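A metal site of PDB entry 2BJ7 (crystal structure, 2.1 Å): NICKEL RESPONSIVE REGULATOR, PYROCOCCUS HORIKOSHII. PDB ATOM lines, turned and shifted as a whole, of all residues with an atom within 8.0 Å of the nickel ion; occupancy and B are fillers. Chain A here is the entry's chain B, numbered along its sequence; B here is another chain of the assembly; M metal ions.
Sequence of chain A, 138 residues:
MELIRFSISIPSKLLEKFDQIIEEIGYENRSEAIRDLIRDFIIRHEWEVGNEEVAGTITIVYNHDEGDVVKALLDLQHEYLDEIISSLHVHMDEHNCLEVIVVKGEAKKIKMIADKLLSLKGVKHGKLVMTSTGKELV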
ATOM      1  N   TYR A  62       0.252   3.810  -1.796  1.00  0.00           N
ATOM      2  CA  TYR A  62      -0.954   3.767  -0.977  1.00  0.00           C
ATOM      3  C   TYR A  62      -1.818   2.558  -1.292  1.00  0.00           C
ATOM      4  O   TYR A  62      -1.608   1.866  -2.291  1.00  0.00           O
ATOM      5  CB  TYR A  62      -1.760   5.046  -1.190  1.00  0.00           C
ATOM      6  CG  TYR A  62      -2.105   5.304  -2.641  1.00  0.00           C
ATOM      7  CD1 TYR A  62      -3.227   4.706  -3.232  1.00  0.00           C
ATOM      8  CD2 TYR A  62      -1.308   6.135  -3.429  1.00  0.00           C
ATOM      9  CE1 TYR A  62      -3.535   4.941  -4.577  1.00  0.00           C
ATOM     10  CE2 TYR A  62      -1.609   6.367  -4.770  1.00  0.00           C
ATOM     11  CZ  TYR A  62      -2.717   5.773  -5.341  1.00  0.00           C
ATOM     12  OH  TYR A  62      -3.011   6.012  -6.666  1.00  0.00           O
ATOM     13  N   ASN A  63      -2.779   2.300  -0.417  1.00  0.00           N
ATOM     14  CA  ASN A  63      -3.713   1.200  -0.595  1.00  0.00           C
ATOM     15  C   ASN A  63      -4.952   1.919  -1.116  1.00  0.00           C
ATOM     16  O   ASN A  63      -5.589   2.683  -0.378  1.00  0.00           O
ATOM     17  CB  ASN A  63      -4.006   0.544   0.754  1.00  0.00           C
ATOM     18  CG  ASN A  63      -5.032  -0.579   0.651  1.00  0.00           C
ATOM     19  OD1 ASN A  63      -6.142  -0.385   0.170  1.00  0.00           O
ATOM     20  ND2 ASN A  63      -4.642  -1.763   1.111  1.00  0.00           N
ATOM     21  N   HIS A  64      -5.282   1.711  -2.389  1.00  0.00           N
ATOM     22  CA  HIS A  64      -6.435   2.391  -2.972  1.00  0.00           C
ATOM     23  C   HIS A  64      -7.761   2.016  -2.333  1.00  0.00           C
ATOM     24  O   HIS A  64      -8.751   2.726  -2.505  1.00  0.00           O
ATOM     25  CB  HIS A  64      -6.511   2.145  -4.476  1.00  0.00           C
ATOM     26  CG  HIS A  64      -6.779   0.725  -4.841  1.00  0.00           C
ATOM     27  ND1 HIS A  64      -5.767  -0.207  -4.992  1.00  0.00           N
ATOM     28  CD2 HIS A  64      -7.931   0.064  -5.083  1.00  0.00           C
ATOM     29  CE1 HIS A  64      -6.299  -1.376  -5.320  1.00  0.00           C
ATOM     30  NE2 HIS A  64      -7.606  -1.236  -5.379  1.00  0.00           N
ATOM     31  N   VAL A  70      -7.862   7.663  -2.477  1.00  0.00           N
ATOM     32  CA  VAL A  70      -7.966   7.787  -3.938  1.00  0.00           C
ATOM     33  C   VAL A  70      -8.690   9.067  -4.360  1.00  0.00           C
ATOM     34  O   VAL A  70      -8.218   9.795  -5.243  1.00  0.00           O
ATOM     35  CB  VAL A  70      -8.705   6.576  -4.552  1.00  0.00           C
ATOM     36  CG1 VAL A  70      -8.941   6.827  -6.042  1.00  0.00           C
ATOM     37  CG2 VAL A  70      -7.894   5.308  -4.360  1.00  0.00           C
ATOM     38  N   HIS A  89       1.216   5.504 -12.904  1.00  0.00           N
ATOM     39  CA  HIS A  89       0.689   4.637 -11.857  1.00  0.00           C
ATOM     40  C   HIS A  89       1.003   3.173 -12.150  1.00  0.00           C
ATOM     41  O   HIS A  89       0.828   2.713 -13.267  1.00  0.00           O
ATOM     42  CB  HIS A  89      -0.824   4.850 -11.741  1.00  0.00           C
ATOM     43  CG  HIS A  89      -1.492   4.005 -10.711  1.00  0.00           C
ATOM     44  ND1 HIS A  89      -2.410   4.518  -9.811  1.00  0.00           N
ATOM     45  CD2 HIS A  89      -1.433   2.669 -10.464  1.00  0.00           C
ATOM     46  CE1 HIS A  89      -2.869   3.539  -9.056  1.00  0.00           C
ATOM     47  NE2 HIS A  89      -2.295   2.406  -9.435  1.00  0.00           N
ATOM     48  N   VAL A  90       1.485   2.474 -11.139  1.00  0.00           N
ATOM     49  CA  VAL A  90       1.811   1.049 -11.251  1.00  0.00           C
ATOM     50  C   VAL A  90       1.073   0.301 -10.152  1.00  0.00           C
ATOM     51  O   VAL A  90       1.152   0.657  -8.982  1.00  0.00           O
ATOM     52  CB  VAL A  90       3.328   0.804 -11.095  1.00  0.00           C
ATOM     53  CG1 VAL A  90       3.611  -0.700 -11.146  1.00  0.00           C
ATOM     54  CG2 VAL A  90       4.100   1.511 -12.194  1.00  0.00           C
ATOM     55  N   HIS A  91       0.325  -0.733 -10.550  1.00  0.00           N
ATOM     56  CA  HIS A  91      -0.421  -1.527  -9.582  1.00  0.00           C
ATOM     57  C   HIS A  91       0.542  -2.549  -8.997  1.00  0.00           C
ATOM     58  O   HIS A  91       0.933  -3.510  -9.672  1.00  0.00           O
ATOM     59  CB  HIS A  91      -1.602  -2.190 -10.274  1.00  0.00           C
ATOM     60  CG  HIS A  91      -2.461  -1.220 -11.039  1.00  0.00           C
ATOM     61  ND1 HIS A  91      -3.080  -0.151 -10.449  1.00  0.00           N
ATOM     62  CD2 HIS A  91      -2.771  -1.155 -12.363  1.00  0.00           C
ATOM     63  CE1 HIS A  91      -3.742   0.536 -11.358  1.00  0.00           C
ATOM     64  NE2 HIS A  91      -3.572  -0.050 -12.528  1.00  0.00           N
ATOM     65  N   MET A  92       0.931  -2.325  -7.748  1.00  0.00           N
ATOM     66  CA  MET A  92       1.884  -3.189  -7.052  1.00  0.00           C
ATOM     67  C   MET A  92       1.337  -4.575  -6.733  1.00  0.00           C
ATOM     68  O   MET A  92       1.949  -5.588  -7.061  1.00  0.00           O
ATOM     69  CB  MET A  92       2.325  -2.503  -5.754  1.00  0.00           C
ATOM     70  CG  MET A  92       3.054  -1.182  -5.970  1.00  0.00           C
ATOM     71  SD  MET A  92       4.758  -1.411  -6.520  1.00  0.00           S
ATOM     72  CE  MET A  92       4.534  -1.727  -8.225  1.00  0.00           C
ATOM     73  N   ASP A  93       0.183  -4.612  -6.093  1.00  0.00           N
ATOM     74  CA  ASP A  93      -0.454  -5.859  -5.744  1.00  0.00           C
ATOM     75  C   ASP A  93      -1.947  -5.594  -5.689  1.00  0.00           C
ATOM     76  O   ASP A  93      -2.408  -4.514  -6.057  1.00  0.00           O
ATOM     77  CB  ASP A  93       0.048  -6.394  -4.391  1.00  0.00           C
ATOM     78  CG  ASP A  93      -0.104  -5.376  -3.273  1.00  0.00           C
ATOM     79  OD1 ASP A  93      -1.237  -4.925  -3.013  1.00  0.00           O
ATOM     80  OD2 ASP A  93       0.916  -5.025  -2.646  1.00  0.00           O
ATOM     81  N   GLU A  94      -2.707  -6.567  -5.220  1.00  0.00           N
ATOM     82  CA  GLU A  94      -4.145  -6.424  -5.147  1.00  0.00           C
ATOM     83  C   GLU A  94      -4.616  -5.120  -4.518  1.00  0.00           C
ATOM     84  O   GLU A  94      -5.608  -4.546  -4.964  1.00  0.00           O
ATOM     85  CB  GLU A  94      -4.767  -7.598  -4.385  1.00  0.00           C
ATOM     86  CG  GLU A  94      -6.276  -7.440  -4.169  1.00  0.00           C
ATOM     87  CD  GLU A  94      -6.885  -8.605  -3.423  1.00  0.00           C
ATOM     88  OE1 GLU A  94      -8.091  -8.537  -3.112  1.00  0.00           O
ATOM     89  OE2 GLU A  94      -6.155  -9.576  -3.145  1.00  0.00           O
ATOM     90  N   HIS A  95      -3.919  -4.646  -3.498  1.00  0.00           N
ATOM     91  CA  HIS A  95      -4.335  -3.428  -2.808  1.00  0.00           C
ATOM     92  C   HIS A  95      -3.423  -2.205  -2.919  1.00  0.00           C
ATOM     93  O   HIS A  95      -3.880  -1.076  -2.809  1.00  0.00           O
ATOM     94  CB  HIS A  95      -4.524  -3.722  -1.314  1.00  0.00           C
ATOM     95  CG  HIS A  95      -5.580  -4.744  -1.032  1.00  0.00           C
ATOM     96  ND1 HIS A  95      -6.907  -4.566  -1.374  1.00  0.00           N
ATOM     97  CD2 HIS A  95      -5.516  -5.945  -0.416  1.00  0.00           C
ATOM     98  CE1 HIS A  95      -7.606  -5.620  -0.992  1.00  0.00           C
ATOM     99  NE2 HIS A  95      -6.792  -6.473  -0.403  1.00  0.00           N
ATOM    100  N   ASN A  96      -2.131  -2.434  -3.145  1.00  0.00           N
ATOM    101  CA  ASN A  96      -1.195  -1.319  -3.200  1.00  0.00           C
ATOM    102  C   ASN A  96      -0.829  -0.766  -4.569  1.00  0.00           C
ATOM    103  O   ASN A  96      -0.532  -1.512  -5.501  1.00  0.00           O
ATOM    104  CB  ASN A  96       0.069  -1.695  -2.440  1.00  0.00           C
ATOM    105  CG  ASN A  96      -0.211  -2.009  -0.988  1.00  0.00           C
ATOM    106  OD1 ASN A  96      -0.733  -1.174  -0.255  1.00  0.00           O
ATOM    107  ND2 ASN A  96       0.142  -3.212  -0.560  1.00  0.00           N
ATOM    108  N   CYS A  97      -0.826   0.553  -4.649  1.00  0.00           N
ATOM    109  CA  CYS A  97      -0.489   1.296  -5.860  1.00  0.00           C
ATOM    110  C   CYS A  97       0.729   2.170  -5.638  1.00  0.00           C
ATOM    111  O   CYS A  97       0.923   2.745  -4.563  1.00  0.00           O
ATOM    112  CB  CYS A  97      -1.645   2.207  -6.262  1.00  0.00           C
ATOM    113  SG  CYS A  97      -3.230   1.426  -6.535  1.00  0.00           S
ATOM    114  N   LEU A  98       1.560   2.284  -6.664  1.00  0.00           N
ATOM    115  CA  LEU A  98       2.718   3.165  -6.618  1.00  0.00           C
ATOM    116  C   LEU A  98       2.384   4.242  -7.646  1.00  0.00           C
ATOM    117  O   LEU A  98       1.981   3.923  -8.769  1.00  0.00           O
ATOM    118  CB  LEU A  98       4.005   2.445  -7.026  1.00  0.00           C
ATOM    119  CG  LEU A  98       5.258   3.336  -6.948  1.00  0.00           C
ATOM    120  CD1 LEU A  98       6.513   2.484  -6.946  1.00  0.00           C
ATOM    121  CD2 LEU A  98       5.274   4.295  -8.131  1.00  0.00           C
ATOM    122  N   GLU A  99       2.541   5.496  -7.280  1.00  0.00           N
ATOM    123  CA  GLU A  99       2.254   6.588  -8.198  1.00  0.00           C
ATOM    124  C   GLU A  99       3.350   7.634  -8.153  1.00  0.00           C
ATOM    125  O   GLU A  99       3.836   7.996  -7.077  1.00  0.00           O
ATOM    126  CB  GLU A  99       0.912   7.236  -7.842  1.00  0.00           C
ATOM    127  CG  GLU A  99       0.406   8.238  -8.875  1.00  0.00           C
ATOM    128  CD  GLU A  99      -0.932   8.862  -8.503  1.00  0.00           C
ATOM    129  OE1 GLU A  99      -1.773   8.167  -7.879  1.00  0.00           O
ATOM    130  OE2 GLU A  99      -1.148  10.045  -8.847  1.00  0.00           O
ATOM    131  N   LEU B  73     -12.547   1.520 -12.041  1.00  0.00           N
ATOM    132  CA  LEU B  73     -11.362   1.426 -12.888  1.00  0.00           C
ATOM    133  C   LEU B  73     -10.195   0.767 -12.157  1.00  0.00           C
ATOM    134  O   LEU B  73      -9.541  -0.128 -12.701  1.00  0.00           O
ATOM    135  CB  LEU B  73     -10.951   2.811 -13.405  1.00  0.00           C
ATOM    136  CG  LEU B  73     -11.770   3.366 -14.575  1.00  0.00           C
ATOM    137  CD1 LEU B  73     -11.477   4.843 -14.771  1.00  0.00           C
ATOM    138  CD2 LEU B  73     -11.472   2.575 -15.854  1.00  0.00           C
ATOM    139  N   LEU B  74      -9.927   1.219 -10.937  1.00  0.00           N
ATOM    140  CA  LEU B  74      -8.835   0.670 -10.141  1.00  0.00           C
ATOM    141  C   LEU B  74      -9.029  -0.801  -9.804  1.00  0.00           C
ATOM    142  O   LEU B  74      -8.112  -1.606  -9.985  1.00  0.00           O
ATOM    143  CB  LEU B  74      -8.685   1.451  -8.837  1.00  0.00           C
ATOM    144  CG  LEU B  74      -7.805   2.707  -8.876  1.00  0.00           C
ATOM    145  CD1 LEU B  74      -7.820   3.373  -7.513  1.00  0.00           C
ATOM    146  CD2 LEU B  74      -6.393   2.325  -9.266  1.00  0.00           C
ATOM    147  N   ASP B  75     -10.209  -1.160  -9.311  1.00  0.00           N
ATOM    148  CA  ASP B  75     -10.495  -2.543  -8.952  1.00  0.00           C
ATOM    149  C   ASP B  75     -10.352  -3.474 -10.164  1.00  0.00           C
ATOM    150  O   ASP B  75      -9.771  -4.548 -10.063  1.00  0.00           O
ATOM    151  CB  ASP B  75     -11.903  -2.658  -8.366  1.00  0.00           C
ATOM    152  CG  ASP B  75     -11.998  -2.089  -6.951  1.00  0.00           C
ATOM    153  OD1 ASP B  75     -13.127  -2.007  -6.420  1.00  0.00           O
ATOM    154  OD2 ASP B  75     -10.952  -1.741  -6.367  1.00  0.00           O
ATOM    155  N   GLN B  77      -8.552  -2.980 -12.875  1.00  0.00           N
ATOM    156  CA  GLN B  77      -7.148  -3.064 -13.275  1.00  0.00           C
ATOM    157  C   GLN B  77      -6.337  -3.916 -12.325  1.00  0.00           C
ATOM    158  O   GLN B  77      -5.449  -4.674 -12.749  1.00  0.00           O
ATOM    159  CB  GLN B  77      -6.529  -1.663 -13.365  1.00  0.00           C
ATOM    160  CG  GLN B  77      -7.106  -0.820 -14.477  1.00  0.00           C
ATOM    161  CD  GLN B  77      -6.386   0.497 -14.640  1.00  0.00           C
ATOM    162  OE1 GLN B  77      -5.176   0.530 -14.838  1.00  0.00           O
ATOM    163  NE2 GLN B  77      -7.133   1.589 -14.562  1.00  0.00           N
ATOM    164  N   HIS B  78      -6.611  -3.796 -11.025  1.00  0.00           N
ATOM    165  CA  HIS B  78      -5.876  -4.585 -10.055  1.00  0.00           C
ATOM    166  C   HIS B  78      -6.173  -6.082 -10.140  1.00  0.00           C
ATOM    167  O   HIS B  78      -5.482  -6.901  -9.533  1.00  0.00           O
ATOM    168  CB  HIS B  78      -6.127  -4.054  -8.649  1.00  0.00           C
ATOM    169  CG  HIS B  78      -5.204  -2.943  -8.269  1.00  0.00           C
ATOM    170  ND1 HIS B  78      -4.178  -3.108  -7.361  1.00  0.00           N
ATOM    171  CD2 HIS B  78      -5.114  -1.670  -8.715  1.00  0.00           C
ATOM    172  CE1 HIS B  78      -3.492  -1.979  -7.264  1.00  0.00           C
ATOM    173  NE2 HIS B  78      -4.040  -1.095  -8.081  1.00  0.00           N
ATOM    174  N   LEU B  81      -3.226  -7.756 -12.798  1.00  0.00           N
ATOM    175  CA  LEU B  81      -1.870  -7.284 -12.537  1.00  0.00           C
ATOM    176  C   LEU B  81      -0.848  -7.828 -13.525  1.00  0.00           C
ATOM    177  O   LEU B  81       0.175  -7.188 -13.779  1.00  0.00           O
ATOM    178  CB  LEU B  81      -1.429  -7.681 -11.125  1.00  0.00           C
ATOM    179  CG  LEU B  81      -2.273  -7.213  -9.932  1.00  0.00           C
ATOM    180  CD1 LEU B  81      -1.714  -7.828  -8.658  1.00  0.00           C
ATOM    181  CD2 LEU B  81      -2.269  -5.693  -9.838  1.00  0.00           C
ATOM    182  N   ILE B  84      -1.627  -5.704 -17.141  1.00  0.00           N
ATOM    183  CA  ILE B  84      -1.443  -4.258 -17.062  1.00  0.00           C
ATOM    184  C   ILE B  84      -0.053  -3.876 -16.553  1.00  0.00           C
ATOM    185  O   ILE B  84       0.314  -4.167 -15.414  1.00  0.00           O
ATOM    186  CB  ILE B  84      -2.528  -3.620 -16.176  1.00  0.00           C
ATOM    187  CG1 ILE B  84      -3.900  -3.867 -16.811  1.00  0.00           C
ATOM    188  CG2 ILE B  84      -2.263  -2.134 -16.005  1.00  0.00           C
ATOM    189  CD1 ILE B  84      -5.060  -3.356 -15.998  1.00  0.00           C
ATOM    190  N   SER B  87       0.024   2.794 -16.104  1.00  0.00           N
ATOM    191  CA  SER B  87      -0.965   3.694 -16.662  1.00  0.00           C
ATOM    192  C   SER B  87      -0.492   5.128 -16.479  1.00  0.00           C
ATOM    193  O   SER B  87       0.091   5.478 -15.448  1.00  0.00           O
ATOM    194  CB  SER B  87      -2.323   3.522 -15.972  1.00  0.00           C
ATOM    195  OG  SER B  87      -2.258   3.892 -14.612  1.00  0.00           O
HETATM  196 NI    NI M   1      -3.148   0.684  -8.684  1.00  0.00          NI
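NE2 of His 91 lies within hydrogen-bond range of OE1 of Gln 77 of chain B (2.9 Å).
O of Ser 87 of chain B is in hydrogen-bond range of N of His 89, at 2.8 Å.
A ring nitrogen (ND1) of His 78 of chain B lies within hydrogen-bond range of the backbone carbonyl oxygen (O) of Asp 93.
O of Glu 94 is in hydrogen-bond range of ND1 of His 78 of chain B, 3.1 Å away.
SG of Cys 97 lies close to ND1 of His 64, 3.4 Å away.
N of Cys 97 is in hydrogen-bond range of O of Tyr 62 (2.8 Å).
Residues that only touch the nickel ion: Leu 74 of chain B (3.7 Å).
Within 4 Å of the nickel ion: His 89, His 91, Cys 97, Leu 74 of chain B and His 78 of chain B.
The nickel ion is bound by ND1 of His 91 (2.0 Å), NE2 of His 89 (2.1 Å), NE2 of His 78 of chain B (2.1 Å) and SG of Cys 97 (2.3 Å).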
